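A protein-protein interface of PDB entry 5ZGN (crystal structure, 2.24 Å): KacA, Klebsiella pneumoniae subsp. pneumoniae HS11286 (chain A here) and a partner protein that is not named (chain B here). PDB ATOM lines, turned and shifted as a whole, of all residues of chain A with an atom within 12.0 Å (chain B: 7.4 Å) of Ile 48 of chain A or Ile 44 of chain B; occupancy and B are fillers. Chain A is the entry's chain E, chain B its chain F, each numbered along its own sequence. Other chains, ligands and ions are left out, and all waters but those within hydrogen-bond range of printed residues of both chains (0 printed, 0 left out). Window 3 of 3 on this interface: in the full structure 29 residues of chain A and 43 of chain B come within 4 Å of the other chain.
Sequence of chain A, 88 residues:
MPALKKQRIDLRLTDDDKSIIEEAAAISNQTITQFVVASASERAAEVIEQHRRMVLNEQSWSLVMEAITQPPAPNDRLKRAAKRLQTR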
ATOM      1  N   VAL A  37     -33.475  14.018 -23.981  1.00  0.00           N
ATOM      2  CA  VAL A  37     -32.848  12.769 -23.552  1.00  0.00           C
ATOM      3  C   VAL A  37     -33.021  11.687 -24.612  1.00  0.00           C
ATOM      4  O   VAL A  37     -32.081  10.944 -24.921  1.00  0.00           O
ATOM      5  CB  VAL A  37     -33.412  12.325 -22.188  1.00  0.00           C
ATOM      6  CG1 VAL A  37     -33.019  10.887 -21.887  1.00  0.00           C
ATOM      7  CG2 VAL A  37     -32.915  13.251 -21.087  1.00  0.00           C
ATOM      8  N   ALA A  38     -34.217  11.589 -25.199  1.00  0.00           N
ATOM      9  CA  ALA A  38     -34.445  10.582 -26.232  1.00  0.00           C
ATOM     10  C   ALA A  38     -33.602  10.861 -27.470  1.00  0.00           C
ATOM     11  O   ALA A  38     -33.043   9.934 -28.068  1.00  0.00           O
ATOM     12  CB  ALA A  38     -35.928  10.518 -26.597  1.00  0.00           C
ATOM     13  N   SER A  39     -33.491  12.130 -27.866  1.00  0.00           N
ATOM     14  CA  SER A  39     -32.685  12.470 -29.033  1.00  0.00           C
ATOM     15  C   SER A  39     -31.209  12.174 -28.793  1.00  0.00           C
ATOM     16  O   SER A  39     -30.518  11.669 -29.687  1.00  0.00           O
ATOM     17  CB  SER A  39     -32.881  13.943 -29.391  1.00  0.00           C
ATOM     18  OG  SER A  39     -34.241  14.231 -29.658  1.00  0.00           O
ATOM     19  N   ALA A  40     -30.706  12.481 -27.597  1.00  0.00           N
ATOM     20  CA  ALA A  40     -29.289  12.282 -27.319  1.00  0.00           C
ATOM     21  C   ALA A  40     -28.956  10.811 -27.097  1.00  0.00           C
ATOM     22  O   ALA A  40     -27.928  10.326 -27.584  1.00  0.00           O
ATOM     23  CB  ALA A  40     -28.867  13.114 -26.107  1.00  0.00           C
ATOM     24  N   SER A  41     -29.812  10.079 -26.378  1.00  0.00           N
ATOM     25  CA  SER A  41     -29.498   8.687 -26.066  1.00  0.00           C
ATOM     26  C   SER A  41     -29.669   7.786 -27.283  1.00  0.00           C
ATOM     27  O   SER A  41     -28.889   6.845 -27.475  1.00  0.00           O
ATOM     28  CB  SER A  41     -30.367   8.197 -24.910  1.00  0.00           C
ATOM     29  OG  SER A  41     -31.739   8.270 -25.242  1.00  0.00           O
ATOM     30  N   GLU A  42     -30.673   8.056 -28.122  1.00  0.00           N
ATOM     31  CA  GLU A  42     -30.795   7.310 -29.372  1.00  0.00           C
ATOM     32  C   GLU A  42     -29.593   7.569 -30.265  1.00  0.00           C
ATOM     33  O   GLU A  42     -29.081   6.652 -30.920  1.00  0.00           O
ATOM     34  CB  GLU A  42     -32.087   7.685 -30.100  1.00  0.00           C
ATOM     35  CG  GLU A  42     -33.345   7.149 -29.444  1.00  0.00           C
ATOM     36  CD  GLU A  42     -34.598   7.470 -30.233  1.00  0.00           C
ATOM     37  OE1 GLU A  42     -35.627   7.797 -29.605  1.00  0.00           O
ATOM     38  OE2 GLU A  42     -34.554   7.398 -31.480  1.00  0.00           O
ATOM     39  N   ARG A  43     -29.125   8.820 -30.294  1.00  0.00           N
ATOM     40  CA  ARG A  43     -27.949   9.158 -31.084  1.00  0.00           C
ATOM     41  C   ARG A  43     -26.676   8.618 -30.450  1.00  0.00           C
ATOM     42  O   ARG A  43     -25.727   8.273 -31.164  1.00  0.00           O
ATOM     43  CB  ARG A  43     -27.863  10.677 -31.262  1.00  0.00           C
ATOM     44  CG  ARG A  43     -26.586  11.114 -31.940  1.00  0.00           C
ATOM     45  CD  ARG A  43     -26.694  10.840 -33.438  1.00  0.00           C
ATOM     46  NE  ARG A  43     -25.533  11.307 -34.162  1.00  0.00           N
ATOM     47  CZ  ARG A  43     -25.136  10.797 -35.326  1.00  0.00           C
ATOM     48  NH1 ARG A  43     -25.803   9.799 -35.903  1.00  0.00           N
ATOM     49  NH2 ARG A  43     -24.051  11.281 -35.926  1.00  0.00           N
ATOM     50  N   ALA A  44     -26.656   8.489 -29.124  1.00  0.00           N
ATOM     51  CA  ALA A  44     -25.531   7.850 -28.450  1.00  0.00           C
ATOM     52  C   ALA A  44     -25.387   6.396 -28.887  1.00  0.00           C
ATOM     53  O   ALA A  44     -24.284   5.938 -29.207  1.00  0.00           O
ATOM     54  CB  ALA A  44     -25.709   7.946 -26.933  1.00  0.00           C
ATOM     55  N   ALA A  45     -26.500   5.655 -28.903  1.00  0.00           N
ATOM     56  CA  ALA A  45     -26.460   4.252 -29.302  1.00  0.00           C
ATOM     57  C   ALA A  45     -25.969   4.082 -30.735  1.00  0.00           C
ATOM     58  O   ALA A  45     -25.319   3.079 -31.050  1.00  0.00           O
ATOM     59  CB  ALA A  45     -27.841   3.619 -29.134  1.00  0.00           C
ATOM     60  N   GLU A  46     -26.269   5.040 -31.616  1.00  0.00           N
ATOM     61  CA  GLU A  46     -25.751   4.976 -32.979  1.00  0.00           C
ATOM     62  C   GLU A  46     -24.235   5.140 -32.998  1.00  0.00           C
ATOM     63  O   GLU A  46     -23.527   4.379 -33.669  1.00  0.00           O
ATOM     64  CB  GLU A  46     -26.413   6.047 -33.846  1.00  0.00           C
ATOM     65  CG  GLU A  46     -27.867   5.768 -34.190  1.00  0.00           C
ATOM     66  CD  GLU A  46     -28.535   6.946 -34.873  1.00  0.00           C
ATOM     67  OE1 GLU A  46     -29.782   6.969 -34.939  1.00  0.00           O
ATOM     68  OE2 GLU A  46     -27.811   7.851 -35.343  1.00  0.00           O
ATOM     69  N   VAL A  47     -23.722   6.132 -32.266  1.00  0.00           N
ATOM     70  CA  VAL A  47     -22.278   6.344 -32.206  1.00  0.00           C
ATOM     71  C   VAL A  47     -21.587   5.123 -31.611  1.00  0.00           C
ATOM     72  O   VAL A  47     -20.560   4.661 -32.124  1.00  0.00           O
ATOM     73  CB  VAL A  47     -21.960   7.622 -31.408  1.00  0.00           C
ATOM     74  CG1 VAL A  47     -20.469   7.721 -31.126  1.00  0.00           C
ATOM     75  CG2 VAL A  47     -22.453   8.851 -32.158  1.00  0.00           C
ATOM     76  N   ILE A  48     -22.151   4.571 -30.537  1.00  0.00           N
ATOM     77  CA  ILE A  48     -21.527   3.434 -29.869  1.00  0.00           C
ATOM     78  C   ILE A  48     -21.531   2.211 -30.778  1.00  0.00           C
ATOM     79  O   ILE A  48     -20.545   1.468 -30.840  1.00  0.00           O
ATOM     80  CB  ILE A  48     -22.224   3.155 -28.525  1.00  0.00           C
ATOM     81  CG1 ILE A  48     -21.983   4.317 -27.558  1.00  0.00           C
ATOM     82  CG2 ILE A  48     -21.729   1.848 -27.924  1.00  0.00           C
ATOM     83  CD1 ILE A  48     -22.762   4.217 -26.265  1.00  0.00           C
ATOM     84  N   GLU A  49     -22.619   1.996 -31.520  1.00  0.00           N
ATOM     85  CA  GLU A  49     -22.696   0.805 -32.358  1.00  0.00           C
ATOM     86  C   GLU A  49     -21.744   0.902 -33.543  1.00  0.00           C
ATOM     87  O   GLU A  49     -21.143  -0.101 -33.942  1.00  0.00           O
ATOM     88  CB  GLU A  49     -24.132   0.592 -32.840  1.00  0.00           C
ATOM     89  N   GLN A  50     -21.570   2.101 -34.104  1.00  0.00           N
ATOM     90  CA  GLN A  50     -20.556   2.293 -35.133  1.00  0.00           C
ATOM     91  C   GLN A  50     -19.146   2.120 -34.583  1.00  0.00           C
ATOM     92  O   GLN A  50     -18.233   1.772 -35.339  1.00  0.00           O
ATOM     93  CB  GLN A  50     -20.711   3.678 -35.773  1.00  0.00           C
ATOM     94  CG  GLN A  50     -19.729   3.969 -36.903  1.00  0.00           C
ATOM     95  CD  GLN A  50     -20.391   3.994 -38.269  1.00  0.00           C
ATOM     96  OE1 GLN A  50     -21.556   4.363 -38.400  1.00  0.00           O
ATOM     97  NE2 GLN A  50     -19.652   3.587 -39.293  1.00  0.00           N
ATOM     98  N   HIS A  51     -18.955   2.330 -33.280  1.00  0.00           N
ATOM     99  CA  HIS A  51     -17.623   2.252 -32.696  1.00  0.00           C
ATOM    100  C   HIS A  51     -17.167   0.812 -32.467  1.00  0.00           C
ATOM    101  O   HIS A  51     -15.963   0.539 -32.511  1.00  0.00           O
ATOM    102  CB  HIS A  51     -17.590   3.043 -31.386  1.00  0.00           C
ATOM    103  CG  HIS A  51     -16.233   3.123 -30.762  1.00  0.00           C
ATOM    104  ND1 HIS A  51     -15.886   2.406 -29.637  1.00  0.00           N
ATOM    105  CD2 HIS A  51     -15.138   3.841 -31.104  1.00  0.00           C
ATOM    106  CE1 HIS A  51     -14.634   2.678 -29.315  1.00  0.00           C
ATOM    107  NE2 HIS A  51     -14.157   3.546 -30.189  1.00  0.00           N
ATOM    108  N   ARG A  52     -18.096  -0.120 -32.232  1.00  0.00           N
ATOM    109  CA  ARG A  52     -17.735  -1.508 -31.952  1.00  0.00           C
ATOM    110  C   ARG A  52     -17.869  -2.439 -33.149  1.00  0.00           C
ATOM    111  O   ARG A  52     -17.280  -3.525 -33.129  1.00  0.00           O
ATOM    112  CB  ARG A  52     -18.603  -2.081 -30.823  1.00  0.00           C
ATOM    113  CG  ARG A  52     -19.159  -1.067 -29.853  1.00  0.00           C
ATOM    114  CD  ARG A  52     -20.576  -1.436 -29.432  1.00  0.00           C
ATOM    115  NE  ARG A  52     -20.735  -1.474 -27.980  1.00  0.00           N
ATOM    116  CZ  ARG A  52     -21.861  -1.810 -27.361  1.00  0.00           C
ATOM    117  NH1 ARG A  52     -22.938  -2.138 -28.065  1.00  0.00           N
ATOM    118  NH2 ARG A  52     -21.913  -1.816 -26.036  1.00  0.00           N
ATOM    119  N   ARG A  53     -18.609  -2.054 -34.182  1.00  0.00           N
ATOM    120  CA  ARG A  53     -18.932  -2.949 -35.286  1.00  0.00           C
ATOM    121  C   ARG A  53     -18.015  -2.656 -36.469  1.00  0.00           C
ATOM    122  O   ARG A  53     -18.116  -1.598 -37.099  1.00  0.00           O
ATOM    123  CB  ARG A  53     -20.404  -2.806 -35.666  1.00  0.00           C
ATOM    124  CG  ARG A  53     -21.340  -3.069 -34.492  1.00  0.00           C
ATOM    125  CD  ARG A  53     -21.963  -4.446 -34.535  1.00  0.00           C
ATOM    126  NE  ARG A  53     -22.780  -4.639 -35.727  1.00  0.00           N
ATOM    127  CZ  ARG A  53     -24.037  -4.219 -35.841  1.00  0.00           C
ATOM    128  NH1 ARG A  53     -24.711  -4.432 -36.965  1.00  0.00           N
ATOM    129  NH2 ARG A  53     -24.622  -3.591 -34.830  1.00  0.00           N
ATOM    130  N   MET A  54     -17.123  -3.595 -36.765  1.00  0.00           N
ATOM    131  CA  MET A  54     -16.244  -3.496 -37.920  1.00  0.00           C
ATOM    132  C   MET A  54     -16.830  -4.289 -39.082  1.00  0.00           C
ATOM    133  O   MET A  54     -16.584  -5.489 -39.203  1.00  0.00           O
ATOM    134  CB  MET A  54     -14.843  -4.024 -37.590  1.00  0.00           C
ATOM    135  CG  MET A  54     -14.380  -3.797 -36.156  1.00  0.00           C
ATOM    136  SD  MET A  54     -13.232  -2.238 -35.930  1.00  0.00           S
ATOM    137  CE  MET A  54     -14.604  -0.849 -35.967  1.00  0.00           C
ATOM    138  N   VAL A  55     -17.614  -3.627 -39.929  1.00  0.00           N
ATOM    139  CA  VAL A  55     -18.157  -4.267 -41.124  1.00  0.00           C
ATOM    140  C   VAL A  55     -17.032  -4.374 -42.147  1.00  0.00           C
ATOM    141  O   VAL A  55     -16.585  -3.368 -42.703  1.00  0.00           O
ATOM    142  CB  VAL A  55     -19.355  -3.497 -41.691  1.00  0.00           C
ATOM    143  CG1 VAL A  55     -19.887  -4.199 -42.930  1.00  0.00           C
ATOM    144  CG2 VAL A  55     -20.447  -3.369 -40.640  1.00  0.00           C
ATOM    145  N   HIS B  40     -15.560   9.904 -18.120  1.00  0.00           N
ATOM    146  CA  HIS B  40     -16.453   9.575 -19.233  1.00  0.00           C
ATOM    147  C   HIS B  40     -16.041   8.231 -19.842  1.00  0.00           C
ATOM    148  O   HIS B  40     -15.737   8.107 -21.028  1.00  0.00           O
ATOM    149  CB  HIS B  40     -16.452  10.682 -20.283  1.00  0.00           C
ATOM    150  CG  HIS B  40     -17.111  11.946 -19.827  1.00  0.00           C
ATOM    151  ND1 HIS B  40     -17.082  13.112 -20.564  1.00  0.00           N
ATOM    152  CD2 HIS B  40     -17.811  12.230 -18.702  1.00  0.00           C
ATOM    153  CE1 HIS B  40     -17.739  14.057 -19.916  1.00  0.00           C
ATOM    154  NE2 HIS B  40     -18.192  13.548 -18.783  1.00  0.00           N
ATOM    155  N   ASP B  41     -16.041   7.211 -18.989  1.00  0.00           N
ATOM    156  CA  ASP B  41     -15.525   5.896 -19.346  1.00  0.00           C
ATOM    157  C   ASP B  41     -15.954   4.899 -18.279  1.00  0.00           C
ATOM    158  O   ASP B  41     -16.496   5.271 -17.235  1.00  0.00           O
ATOM    159  CB  ASP B  41     -14.001   5.913 -19.486  1.00  0.00           C
ATOM    160  CG  ASP B  41     -13.314   6.553 -18.294  1.00  0.00           C
ATOM    161  OD1 ASP B  41     -13.229   5.902 -17.231  1.00  0.00           O
ATOM    162  OD2 ASP B  41     -12.854   7.707 -18.424  1.00  0.00           O
ATOM    163  N   GLY B  42     -15.722   3.618 -18.571  1.00  0.00           N
ATOM    164  CA  GLY B  42     -16.003   2.528 -17.652  1.00  0.00           C
ATOM    165  C   GLY B  42     -16.948   1.489 -18.210  1.00  0.00           C
ATOM    166  O   GLY B  42     -16.888   0.321 -17.809  1.00  0.00           O
ATOM    167  N   GLN B  43     -17.817   1.881 -19.142  1.00  0.00           N
ATOM    168  CA  GLN B  43     -18.806   0.982 -19.720  1.00  0.00           C
ATOM    169  C   GLN B  43     -18.496   0.572 -21.154  1.00  0.00           C
ATOM    170  O   GLN B  43     -18.681  -0.596 -21.507  1.00  0.00           O
ATOM    171  CB  GLN B  43     -20.194   1.629 -19.648  1.00  0.00           C
ATOM    172  CG  GLN B  43     -20.489   2.332 -18.315  1.00  0.00           C
ATOM    173  CD  GLN B  43     -20.379   1.401 -17.116  1.00  0.00           C
ATOM    174  OE1 GLN B  43     -19.338   1.323 -16.468  1.00  0.00           O
ATOM    175  NE2 GLN B  43     -21.450   0.672 -16.836  1.00  0.00           N
ATOM    176  N   ILE B  44     -18.010   1.494 -21.988  1.00  0.00           N
ATOM    177  CA  ILE B  44     -17.609   1.199 -23.356  1.00  0.00           C
ATOM    178  C   ILE B  44     -16.137   1.485 -23.578  1.00  0.00           C
ATOM    179  O   ILE B  44     -15.435   0.713 -24.246  1.00  0.00           O
ATOM    180  CB  ILE B  44     -18.472   1.981 -24.372  1.00  0.00           C
ATOM    181  CG1 ILE B  44     -19.945   1.627 -24.191  1.00  0.00           C
ATOM    182  CG2 ILE B  44     -17.999   1.706 -25.804  1.00  0.00           C
ATOM    183  CD1 ILE B  44     -20.738   2.687 -23.448  1.00  0.00           C
ATOM    184  N   LEU B  45     -15.636   2.583 -23.021  1.00  0.00           N
ATOM    185  CA  LEU B  45     -14.232   2.939 -23.127  1.00  0.00           C
ATOM    186  C   LEU B  45     -13.519   2.638 -21.814  1.00  0.00           C
ATOM    187  O   LEU B  45     -14.009   2.975 -20.731  1.00  0.00           O
ATOM    188  CB  LEU B  45     -14.067   4.420 -23.476  1.00  0.00           C
ATOM    189  CG  LEU B  45     -14.725   4.936 -24.758  1.00  0.00           C
ATOM    190  CD1 LEU B  45     -14.884   6.451 -24.707  1.00  0.00           C
ATOM    191  CD2 LEU B  45     -13.938   4.520 -25.993  1.00  0.00           C
ATOM    192  N   ARG B  46     -12.354   2.006 -21.924  1.00  0.00           N
ATOM    193  CA  ARG B  46     -11.500   1.698 -20.786  1.00  0.00           C
ATOM    194  C   ARG B  46     -10.142   2.331 -21.036  1.00  0.00           C
ATOM    195  O   ARG B  46      -9.516   2.078 -22.072  1.00  0.00           O
ATOM    196  CB  ARG B  46     -11.367   0.190 -20.571  1.00  0.00           C
ATOM    197  CG  ARG B  46     -10.537  -0.198 -19.347  1.00  0.00           C
ATOM    198  CD  ARG B  46     -11.422  -0.497 -18.120  1.00  0.00           C
ATOM    199  NE  ARG B  46     -11.634   0.688 -17.304  1.00  0.00           N
ATOM    200  CZ  ARG B  46     -12.631   0.844 -16.436  1.00  0.00           C
ATOM    201  NH1 ARG B  46     -13.534  -0.113 -16.251  1.00  0.00           N
ATOM    202  NH2 ARG B  46     -12.724   1.972 -15.736  1.00  0.00           N
ATOM    203  N   THR B  64      -7.146   4.378 -24.856  1.00  0.00           N
ATOM    204  CA  THR B  64      -8.495   3.900 -24.601  1.00  0.00           C
ATOM    205  C   THR B  64      -8.721   2.597 -25.353  1.00  0.00           C
ATOM    206  O   THR B  64      -8.325   2.461 -26.516  1.00  0.00           O
ATOM    207  CB  THR B  64      -9.544   4.934 -25.026  1.00  0.00           C
ATOM    208  OG1 THR B  64      -9.324   5.303 -26.393  1.00  0.00           O
ATOM    209  CG2 THR B  64      -9.446   6.175 -24.152  1.00  0.00           C
ATOM    210  N   LEU B  65      -9.358   1.643 -24.682  1.00  0.00           N
ATOM    211  CA  LEU B  65      -9.702   0.357 -25.266  1.00  0.00           C
ATOM    212  C   LEU B  65     -11.207   0.146 -25.199  1.00  0.00           C
ATOM    213  O   LEU B  65     -11.880   0.632 -24.285  1.00  0.00           O
ATOM    214  CB  LEU B  65      -8.993  -0.799 -24.549  1.00  0.00           C
ATOM    215  CG  LEU B  65      -7.539  -1.059 -24.931  1.00  0.00           C
ATOM    216  CD1 LEU B  65      -6.993  -2.275 -24.198  1.00  0.00           C
ATOM    217  CD2 LEU B  65      -7.420  -1.237 -26.428  1.00  0.00           C
ATOM    218  N   SER B  66     -11.728  -0.590 -26.175  1.00  0.00           N
ATOM    219  CA  SER B  66     -13.150  -0.889 -26.225  1.00  0.00           C
ATOM    220  C   SER B  66     -13.349  -2.270 -26.824  1.00  0.00           C
ATOM    221  O   SER B  66     -12.666  -2.643 -27.781  1.00  0.00           O
ATOM    222  CB  SER B  66     -13.915   0.152 -27.047  1.00  0.00           C
ATOM    223  OG  SER B  66     -13.781   1.440 -26.481  1.00  0.00           O
ATOM    224  N   GLY B  67     -14.282  -3.023 -26.251  1.00  0.00           N
ATOM    225  CA  GLY B  67     -14.688  -4.266 -26.879  1.00  0.00           C
ATOM    226  C   GLY B  67     -15.323  -3.997 -28.231  1.00  0.00           C
ATOM    227  O   GLY B  67     -16.068  -3.031 -28.410  1.00  0.00           O
ATOM    228  N   THR B  93     -10.650  -3.124 -29.875  1.00  0.00           N
ATOM    229  CA  THR B  93     -10.243  -2.003 -30.708  1.00  0.00           C
ATOM    230  C   THR B  93      -9.541  -0.956 -29.856  1.00  0.00           C
ATOM    231  O   THR B  93     -10.090  -0.496 -28.848  1.00  0.00           O
ATOM    232  CB  THR B  93     -11.446  -1.385 -31.425  1.00  0.00           C
ATOM    233  OG1 THR B  93     -11.893  -2.275 -32.453  1.00  0.00           O
ATOM    234  CG2 THR B  93     -11.074  -0.047 -32.050  1.00  0.00           C
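Ile 44 of chain B touches Ile 48 of chain A (CD1 to CD1, 3.8 Å). His 51 of chain A touches Leu 45 of chain B (CE1 to CD2, 3.9 Å). His 51 of chain A touches Ser 66 of chain B (CE1 to OG, 3.2 Å). CB of Arg 52 of chain A touches O of Gly 67 of chain B (3.6 Å).
Ala 40 of chain A touches none of the printed residues of chain B. Ile 48 of chain A touches just one residue of chain B: Ile 44. Of the printed residues of chain B, His 51 of chain A touches Leu 45 (3.9 Å) and Ser 66 (3.2 Å). Of the printed residues of chain B, Met 54 of chain A touches Thr 93. Val 55 of chain A touches none of the printed residues of chain B. No residue of chain A comes within 4 Å of Gln 43 of chain B. Ile 44 of chain B touches one residue of chain A. Gly 67 of chain B touches one residue of chain A. Of the printed residues of chain A, Thr 93 of chain B touches Met 54. The nearest residue of chain B that does not touch Ile 48 of chain A is Gly 67 of chain B (6.8 Å).
The side-chain sulfur (SD) of Met 54 of chain A lies within hydrogen-bond range of the side-chain hydroxyl (OG1) of Thr 93 of chain B.
Hydrophobic or aromatic side chains of chain B within 4 Å of the printed part of chain A: Ile 44 and Leu 45. Among the printed residues, 5 pairs touch across the chains. Among the printed residues, no Asp or Glu carboxylate lies within 4 Å of a Lys or Arg side-chain nitrogen of the other chain.
O of Ile 44 of chain B sits at hydrogen-bond distance from OG of Ser 66 of chain B (2.9 Å). The backbone carbonyl oxygen (O) of Ser 66 of chain B sits at hydrogen-bond distance from the backbone NH (N) of Thr 93 of chain B (2.9 Å).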
